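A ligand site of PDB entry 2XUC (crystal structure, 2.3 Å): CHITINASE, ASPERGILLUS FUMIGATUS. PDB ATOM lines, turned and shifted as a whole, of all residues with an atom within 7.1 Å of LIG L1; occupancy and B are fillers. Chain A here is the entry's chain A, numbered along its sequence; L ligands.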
ATOM      1  N   TYR A   7      10.880 -29.259 -24.273  1.00  0.00           N
ATOM      2  CA  TYR A   7      11.976 -29.983 -23.637  1.00  0.00           C
ATOM      3  C   TYR A   7      11.382 -30.945 -22.634  1.00  0.00           C
ATOM      4  O   TYR A   7      10.381 -30.619 -21.975  1.00  0.00           O
ATOM      5  CB  TYR A   7      12.932 -29.017 -22.928  1.00  0.00           C
ATOM      6  CG  TYR A   7      13.958 -28.419 -23.895  1.00  0.00           C
ATOM      7  CD1 TYR A   7      13.622 -27.346 -24.718  1.00  0.00           C
ATOM      8  CD2 TYR A   7      15.262 -28.942 -23.981  1.00  0.00           C
ATOM      9  CE1 TYR A   7      14.584 -26.787 -25.643  1.00  0.00           C
ATOM     10  CE2 TYR A   7      16.204 -28.420 -24.907  1.00  0.00           C
ATOM     11  CZ  TYR A   7      15.866 -27.317 -25.710  1.00  0.00           C
ATOM     12  OH  TYR A   7      16.769 -26.786 -26.614  1.00  0.00           O
ATOM     13  N   ASN A  30      12.593 -32.147 -27.480  1.00  0.00           N
ATOM     14  CA  ASN A  30      14.020 -32.170 -27.250  1.00  0.00           C
ATOM     15  C   ASN A  30      14.272 -32.851 -25.922  1.00  0.00           C
ATOM     16  O   ASN A  30      13.671 -32.458 -24.911  1.00  0.00           O
ATOM     17  CB  ASN A  30      14.551 -30.738 -27.232  1.00  0.00           C
ATOM     18  CG  ASN A  30      14.222 -29.976 -28.526  1.00  0.00           C
ATOM     19  OD1 ASN A  30      14.407 -30.467 -29.626  1.00  0.00           O
ATOM     20  ND2 ASN A  30      13.827 -28.733 -28.363  1.00  0.00           N
ATOM     21  N   PHE A  33      19.673 -34.250 -20.836  1.00  0.00           N
ATOM     22  CA  PHE A  33      20.730 -33.670 -21.690  1.00  0.00           C
ATOM     23  C   PHE A  33      21.904 -34.606 -21.747  1.00  0.00           C
ATOM     24  O   PHE A  33      22.080 -35.448 -20.874  1.00  0.00           O
ATOM     25  CB  PHE A  33      21.251 -32.377 -21.051  1.00  0.00           C
ATOM     26  CG  PHE A  33      20.293 -31.259 -21.141  1.00  0.00           C
ATOM     27  CD1 PHE A  33      20.108 -30.650 -22.354  1.00  0.00           C
ATOM     28  CD2 PHE A  33      19.494 -30.881 -20.038  1.00  0.00           C
ATOM     29  CE1 PHE A  33      19.149 -29.616 -22.484  1.00  0.00           C
ATOM     30  CE2 PHE A  33      18.575 -29.864 -20.146  1.00  0.00           C
ATOM     31  CZ  PHE A  33      18.418 -29.195 -21.372  1.00  0.00           C
ATOM     32  N   SER A  93      19.288 -33.505 -26.887  1.00  0.00           N
ATOM     33  CA  SER A  93      19.824 -32.220 -26.561  1.00  0.00           C
ATOM     34  C   SER A  93      21.172 -32.273 -25.861  1.00  0.00           C
ATOM     35  O   SER A  93      21.406 -33.132 -25.001  1.00  0.00           O
ATOM     36  CB  SER A  93      18.829 -31.461 -25.700  1.00  0.00           C
ATOM     37  OG  SER A  93      19.240 -30.143 -25.624  1.00  0.00           O
ATOM     38  N   GLY A  96      22.553 -28.057 -21.632  1.00  0.00           N
ATOM     39  CA  GLY A  96      21.672 -27.618 -20.530  1.00  0.00           C
ATOM     40  C   GLY A  96      22.413 -26.769 -19.484  1.00  0.00           C
ATOM     41  O   GLY A  96      23.537 -26.322 -19.733  1.00  0.00           O
ATOM     42  N   ALA A  97      21.835 -26.618 -18.291  1.00  0.00           N
ATOM     43  CA  ALA A  97      22.394 -25.764 -17.223  1.00  0.00           C
ATOM     44  C   ALA A  97      23.453 -26.379 -16.290  1.00  0.00           C
ATOM     45  O   ALA A  97      24.321 -25.664 -15.797  1.00  0.00           O
ATOM     46  CB  ALA A  97      21.304 -25.213 -16.374  1.00  0.00           C
ATOM     47  N   TYR A  98      23.342 -27.669 -16.005  1.00  0.00           N
ATOM     48  CA  TYR A  98      24.186 -28.292 -15.019  1.00  0.00           C
ATOM     49  C   TYR A  98      24.898 -29.485 -15.643  1.00  0.00           C
ATOM     50  O   TYR A  98      24.272 -30.317 -16.279  1.00  0.00           O
ATOM     51  CB  TYR A  98      23.395 -28.693 -13.746  1.00  0.00           C
ATOM     52  CG  TYR A  98      24.313 -29.328 -12.711  1.00  0.00           C
ATOM     53  CD1 TYR A  98      24.507 -30.715 -12.697  1.00  0.00           C
ATOM     54  CD2 TYR A  98      25.042 -28.541 -11.785  1.00  0.00           C
ATOM     55  CE1 TYR A  98      25.383 -31.304 -11.779  1.00  0.00           C
ATOM     56  CE2 TYR A  98      25.913 -29.142 -10.860  1.00  0.00           C
ATOM     57  CZ  TYR A  98      26.077 -30.521 -10.865  1.00  0.00           C
ATOM     58  OH  TYR A  98      26.932 -31.131  -9.964  1.00  0.00           O
ATOM     59  N   ASP A 143      20.151 -31.290 -30.655  1.00  0.00           N
ATOM     60  CA  ASP A 143      19.891 -29.949 -30.190  1.00  0.00           C
ATOM     61  C   ASP A 143      21.068 -29.469 -29.351  1.00  0.00           C
ATOM     62  O   ASP A 143      21.592 -30.229 -28.507  1.00  0.00           O
ATOM     63  CB  ASP A 143      18.591 -29.924 -29.383  1.00  0.00           C
ATOM     64  CG  ASP A 143      18.315 -28.572 -28.742  1.00  0.00           C
ATOM     65  OD1 ASP A 143      17.944 -27.637 -29.470  1.00  0.00           O
ATOM     66  OD2 ASP A 143      18.462 -28.437 -27.493  1.00  0.00           O
ATOM     67  N   ASP A 145      22.081 -26.909 -26.743  1.00  0.00           N
ATOM     68  CA  ASP A 145      21.634 -26.081 -25.658  1.00  0.00           C
ATOM     69  C   ASP A 145      22.848 -25.781 -24.782  1.00  0.00           C
ATOM     70  O   ASP A 145      22.877 -26.123 -23.600  1.00  0.00           O
ATOM     71  CB  ASP A 145      20.543 -26.754 -24.833  1.00  0.00           C
ATOM     72  CG  ASP A 145      20.019 -25.845 -23.714  1.00  0.00           C
ATOM     73  OD1 ASP A 145      20.235 -24.576 -23.794  1.00  0.00           O
ATOM     74  OD2 ASP A 145      19.402 -26.358 -22.738  1.00  0.00           O
ATOM     75  N   GLU A 147      25.029 -23.421 -22.692  1.00  0.00           N
ATOM     76  CA  GLU A 147      24.651 -22.264 -21.849  1.00  0.00           C
ATOM     77  C   GLU A 147      25.806 -21.596 -21.123  1.00  0.00           C
ATOM     78  O   GLU A 147      25.614 -20.635 -20.371  1.00  0.00           O
ATOM     79  CB  GLU A 147      23.522 -22.633 -20.846  1.00  0.00           C
ATOM     80  CG  GLU A 147      22.233 -23.090 -21.596  1.00  0.00           C
ATOM     81  CD  GLU A 147      21.011 -23.367 -20.733  1.00  0.00           C
ATOM     82  OE1 GLU A 147      21.075 -23.226 -19.519  1.00  0.00           O
ATOM     83  OE2 GLU A 147      19.969 -23.761 -21.290  1.00  0.00           O
ATOM     84  N   ALA A 178      19.496 -23.662 -29.107  1.00  0.00           N
ATOM     85  CA  ALA A 178      18.759 -22.939 -28.083  1.00  0.00           C
ATOM     86  C   ALA A 178      19.494 -21.764 -27.447  1.00  0.00           C
ATOM     87  O   ALA A 178      19.749 -21.823 -26.216  1.00  0.00           O
ATOM     88  CB  ALA A 178      18.379 -23.903 -26.925  1.00  0.00           C
ATOM     89  N   GLN A 180      20.251 -17.897 -25.856  1.00  0.00           N
ATOM     90  CA  GLN A 180      19.617 -16.904 -25.037  1.00  0.00           C
ATOM     91  C   GLN A 180      19.488 -15.615 -25.831  1.00  0.00           C
ATOM     92  O   GLN A 180      19.983 -15.533 -26.955  1.00  0.00           O
ATOM     93  CB  GLN A 180      20.352 -16.729 -23.699  1.00  0.00           C
ATOM     94  CG  GLN A 180      20.199 -17.997 -22.842  1.00  0.00           C
ATOM     95  CD  GLN A 180      21.072 -18.027 -21.566  1.00  0.00           C
ATOM     96  OE1 GLN A 180      22.312 -18.183 -21.623  1.00  0.00           O
ATOM     97  NE2 GLN A 180      20.426 -17.944 -20.424  1.00  0.00           N
ATOM     98  N   TRP A 201      15.466 -21.998 -31.400  1.00  0.00           N
ATOM     99  CA  TRP A 201      14.528 -21.540 -30.437  1.00  0.00           C
ATOM    100  C   TRP A 201      15.299 -20.637 -29.496  1.00  0.00           C
ATOM    101  O   TRP A 201      16.134 -21.114 -28.754  1.00  0.00           O
ATOM    102  CB  TRP A 201      13.882 -22.660 -29.621  1.00  0.00           C
ATOM    103  CG  TRP A 201      14.432 -24.011 -29.818  1.00  0.00           C
ATOM    104  CD1 TRP A 201      15.548 -24.593 -29.179  1.00  0.00           C
ATOM    105  CD2 TRP A 201      13.908 -25.000 -30.710  1.00  0.00           C
ATOM    106  NE1 TRP A 201      15.720 -25.893 -29.667  1.00  0.00           N
ATOM    107  CE2 TRP A 201      14.739 -26.160 -30.601  1.00  0.00           C
ATOM    108  CE3 TRP A 201      12.829 -25.009 -31.629  1.00  0.00           C
ATOM    109  CZ2 TRP A 201      14.510 -27.329 -31.344  1.00  0.00           C
ATOM    110  CZ3 TRP A 201      12.595 -26.186 -32.387  1.00  0.00           C
ATOM    111  CH2 TRP A 201      13.428 -27.358 -32.199  1.00  0.00           C
ATOM    112  N   GLN A 203      15.765 -18.666 -26.292  1.00  0.00           N
ATOM    113  CA  GLN A 203      15.163 -18.700 -24.965  1.00  0.00           C
ATOM    114  C   GLN A 203      14.841 -17.265 -24.578  1.00  0.00           C
ATOM    115  O   GLN A 203      15.789 -16.468 -24.371  1.00  0.00           O
ATOM    116  CB  GLN A 203      16.163 -19.274 -23.942  1.00  0.00           C
ATOM    117  CG  GLN A 203      16.502 -20.761 -24.180  1.00  0.00           C
ATOM    118  CD  GLN A 203      17.425 -21.313 -23.135  1.00  0.00           C
ATOM    119  OE1 GLN A 203      17.043 -21.405 -21.978  1.00  0.00           O
ATOM    120  NE2 GLN A 203      18.633 -21.734 -23.542  1.00  0.00           N
ATOM    121  N   TYR A 205      13.435 -16.060 -21.791  1.00  0.00           N
ATOM    122  CA  TYR A 205      13.252 -16.021 -20.317  1.00  0.00           C
ATOM    123  C   TYR A 205      14.607 -16.089 -19.680  1.00  0.00           C
ATOM    124  O   TYR A 205      15.559 -16.621 -20.294  1.00  0.00           O
ATOM    125  CB  TYR A 205      12.445 -17.213 -19.787  1.00  0.00           C
ATOM    126  CG  TYR A 205      12.821 -18.539 -20.457  1.00  0.00           C
ATOM    127  CD1 TYR A 205      12.230 -18.918 -21.684  1.00  0.00           C
ATOM    128  CD2 TYR A 205      13.776 -19.365 -19.909  1.00  0.00           C
ATOM    129  CE1 TYR A 205      12.586 -20.074 -22.315  1.00  0.00           C
ATOM    130  CE2 TYR A 205      14.137 -20.573 -20.537  1.00  0.00           C
ATOM    131  CZ  TYR A 205      13.551 -20.899 -21.758  1.00  0.00           C
ATOM    132  OH  TYR A 205      13.929 -22.048 -22.408  1.00  0.00           O
ATOM    133  N   ASN A 206      14.664 -15.631 -18.419  1.00  0.00           N
ATOM    134  CA  ASN A 206      15.882 -15.601 -17.587  1.00  0.00           C
ATOM    135  C   ASN A 206      16.885 -14.476 -17.867  1.00  0.00           C
ATOM    136  O   ASN A 206      17.759 -14.244 -17.034  1.00  0.00           O
ATOM    137  CB  ASN A 206      16.570 -16.963 -17.476  1.00  0.00           C
ATOM    138  CG  ASN A 206      15.731 -17.972 -16.681  1.00  0.00           C
ATOM    139  OD1 ASN A 206      14.859 -17.564 -15.891  1.00  0.00           O
ATOM    140  ND2 ASN A 206      15.975 -19.251 -16.887  1.00  0.00           N
ATOM    141  N   LEU A 246       9.651 -20.135 -24.488  1.00  0.00           N
ATOM    142  CA  LEU A 246       8.907 -19.601 -23.326  1.00  0.00           C
ATOM    143  C   LEU A 246       8.871 -20.574 -22.150  1.00  0.00           C
ATOM    144  O   LEU A 246       8.909 -21.789 -22.363  1.00  0.00           O
ATOM    145  CB  LEU A 246       7.460 -19.278 -23.739  1.00  0.00           C
ATOM    146  CG  LEU A 246       7.264 -18.192 -24.842  1.00  0.00           C
ATOM    147  CD1 LEU A 246       5.785 -18.214 -25.214  1.00  0.00           C
ATOM    148  CD2 LEU A 246       7.692 -16.809 -24.343  1.00  0.00           C
ATOM    149  N   ALA A 252       8.847 -22.485 -13.998  1.00  0.00           N
ATOM    150  CA  ALA A 252       9.742 -23.151 -14.957  1.00  0.00           C
ATOM    151  C   ALA A 252      11.024 -22.371 -15.198  1.00  0.00           C
ATOM    152  O   ALA A 252      11.979 -22.907 -15.689  1.00  0.00           O
ATOM    153  CB  ALA A 252       9.018 -23.367 -16.312  1.00  0.00           C
ATOM    154  N   ALA A 253      10.990 -21.081 -14.903  1.00  0.00           N
ATOM    155  CA  ALA A 253      12.134 -20.149 -15.002  1.00  0.00           C
ATOM    156  C   ALA A 253      12.014 -19.153 -13.846  1.00  0.00           C
ATOM    157  O   ALA A 253      11.024 -19.181 -13.095  1.00  0.00           O
ATOM    158  CB  ALA A 253      12.024 -19.388 -16.318  1.00  0.00           C
ATOM    159  N   MET A 283       8.756 -22.727 -28.637  1.00  0.00           N
ATOM    160  CA  MET A 283       9.406 -23.739 -27.854  1.00  0.00           C
ATOM    161  C   MET A 283       9.030 -23.484 -26.400  1.00  0.00           C
ATOM    162  O   MET A 283       8.880 -22.336 -25.965  1.00  0.00           O
ATOM    163  CB  MET A 283      10.928 -23.681 -28.044  1.00  0.00           C
ATOM    164  CG  MET A 283      11.771 -24.666 -27.154  1.00  0.00           C
ATOM    165  SD  MET A 283      12.057 -23.925 -25.506  1.00  0.00           S
ATOM    166  CE  MET A 283      13.588 -23.066 -25.834  1.00  0.00           C
ATOM    167  N   LEU A 284       8.909 -24.565 -25.655  1.00  0.00           N
ATOM    168  CA  LEU A 284       8.514 -24.507 -24.250  1.00  0.00           C
ATOM    169  C   LEU A 284       9.510 -25.200 -23.337  1.00  0.00           C
ATOM    170  O   LEU A 284       9.906 -26.347 -23.554  1.00  0.00           O
ATOM    171  CB  LEU A 284       7.110 -25.095 -23.987  1.00  0.00           C
ATOM    172  CG  LEU A 284       5.935 -24.232 -24.428  1.00  0.00           C
ATOM    173  CD1 LEU A 284       4.626 -25.044 -24.282  1.00  0.00           C
ATOM    174  CD2 LEU A 284       5.855 -22.849 -23.729  1.00  0.00           C
ATOM    175  N   TRP A 285       9.884 -24.467 -22.298  1.00  0.00           N
ATOM    176  CA  TRP A 285      10.690 -25.046 -21.205  1.00  0.00           C
ATOM    177  C   TRP A 285       9.715 -25.095 -20.036  1.00  0.00           C
ATOM    178  O   TRP A 285       9.319 -24.024 -19.564  1.00  0.00           O
ATOM    179  CB  TRP A 285      11.951 -24.190 -20.888  1.00  0.00           C
ATOM    180  CG  TRP A 285      12.686 -24.780 -19.669  1.00  0.00           C
ATOM    181  CD1 TRP A 285      12.545 -24.393 -18.364  1.00  0.00           C
ATOM    182  CD2 TRP A 285      13.564 -25.919 -19.669  1.00  0.00           C
ATOM    183  NE1 TRP A 285      13.306 -25.217 -17.552  1.00  0.00           N
ATOM    184  CE2 TRP A 285      13.939 -26.155 -18.323  1.00  0.00           C
ATOM    185  CE3 TRP A 285      14.074 -26.765 -20.693  1.00  0.00           C
ATOM    186  CZ2 TRP A 285      14.790 -27.220 -17.951  1.00  0.00           C
ATOM    187  CZ3 TRP A 285      14.940 -27.817 -20.319  1.00  0.00           C
ATOM    188  CH2 TRP A 285      15.274 -28.039 -18.959  1.00  0.00           C
ATOM    189  N   GLU A 286       9.228 -26.284 -19.622  1.00  0.00           N
ATOM    190  CA  GLU A 286       9.473 -27.607 -20.219  1.00  0.00           C
ATOM    191  C   GLU A 286       8.270 -28.539 -19.943  1.00  0.00           C
ATOM    192  O   GLU A 286       7.253 -28.106 -19.400  1.00  0.00           O
ATOM    193  CB  GLU A 286      10.803 -28.203 -19.696  1.00  0.00           C
ATOM    194  CG  GLU A 286      10.896 -28.312 -18.171  1.00  0.00           C
ATOM    195  CD  GLU A 286      10.252 -29.580 -17.648  1.00  0.00           C
ATOM    196  OE1 GLU A 286      10.691 -30.681 -18.019  1.00  0.00           O
ATOM    197  OE2 GLU A 286       9.279 -29.506 -16.893  1.00  0.00           O
HETATM  198  C1  LIG L   1      16.035 -24.841 -23.344  1.00  0.00           C
HETATM  199  N1  LIG L   1      17.104 -24.615 -22.387  1.00  0.00           N
HETATM  200  C2  LIG L   1      16.667 -24.153 -21.218  1.00  0.00           C
HETATM  201  O1  LIG L   1      15.478 -23.881 -20.986  1.00  0.00           O
HETATM  202  N2  LIG L   1      17.621 -23.946 -20.284  1.00  0.00           N
HETATM  203  C3  LIG L   1      17.406 -23.435 -19.083  1.00  0.00           C
HETATM  204  N3  LIG L   1      16.176 -23.231 -18.661  1.00  0.00           N
HETATM  205  N4  LIG L   1      18.434 -23.143 -18.293  1.00  0.00           N
HETATM  206  C4  LIG L   1      18.156 -22.614 -16.901  1.00  0.00           C
HETATM  207  C1  LG2 L   2      21.139 -32.254 -14.533  1.00  0.00           C
HETATM  208  N1  LG2 L   2      20.887 -31.178 -15.529  1.00  0.00           N
HETATM  209  C2  LG2 L   2      19.864 -30.321 -15.337  1.00  0.00           C
HETATM  210  O1  LG2 L   2      19.050 -30.403 -14.385  1.00  0.00           O
HETATM  211  N2  LG2 L   2      19.772 -29.350 -16.317  1.00  0.00           N
HETATM  212  C3  LG2 L   2      18.856 -28.376 -16.466  1.00  0.00           C
HETATM  213  N3  LG2 L   2      17.844 -28.224 -15.621  1.00  0.00           N
HETATM  214  N4  LG2 L   2      19.002 -27.514 -17.482  1.00  0.00           N
HETATM  215  C4  LG2 L   2      18.000 -26.441 -17.656  1.00  0.00           C
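The side-chain carboxylate of Glu 147 is in hydrogen-bond range of a nitrogen (N4) of LIG L1, at 2.9 Å. The side-chain hydroxyl (OH) of Tyr 205 sits at hydrogen-bond distance from an oxygen (O1) of LIG L1, 2.8 Å away. An oxygen (O1) of LIG L1 lies close to the side-chain amide oxygen (OE1) of Gln 203. The side-chain carboxylate (OD2) of Asp 145 is in hydrogen-bond range of a nitrogen (N1) of LIG L1, at 2.9 Å.
The side-chain amide nitrogen (NE2) of Gln 203 is in hydrogen-bond range of the side-chain carboxylate (OE2) of Glu 147, 3.3 Å away. OE2 of Glu 147 lies close to OD1 of Asp 145. OD1 of Asp 145 is in hydrogen-bond range of NE2 of Gln 203 (3.3 Å). O of Ala 178 sits at hydrogen-bond distance from NE2 of Gln 203 (2.9 Å). The backbone carbonyl oxygen of Leu 246 lies within hydrogen-bond range of the backbone NH of Trp 285, 2.9 Å away. The side-chain hydroxyl (OH) of Tyr 7 sits at hydrogen-bond distance from the side-chain carboxylate (OD2) of Asp 143 (2.5 Å). The backbone NH (N) of Tyr 7 is in hydrogen-bond range of the backbone carbonyl oxygen (O) of Leu 284 (3.2 Å). The backbone carbonyl oxygen (O) of Met 283 is in hydrogen-bond range of the backbone NH (N) of Leu 246 (2.8 Å).
Residues that only touch LIG L1: Tyr 7, Met 283 and Trp 285. Of the 23 residues printed, 7 come within 4 Å of LIG L1. The nearest printed residue that does not touch LIG L1 is Asn 206 (4.01 Å).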
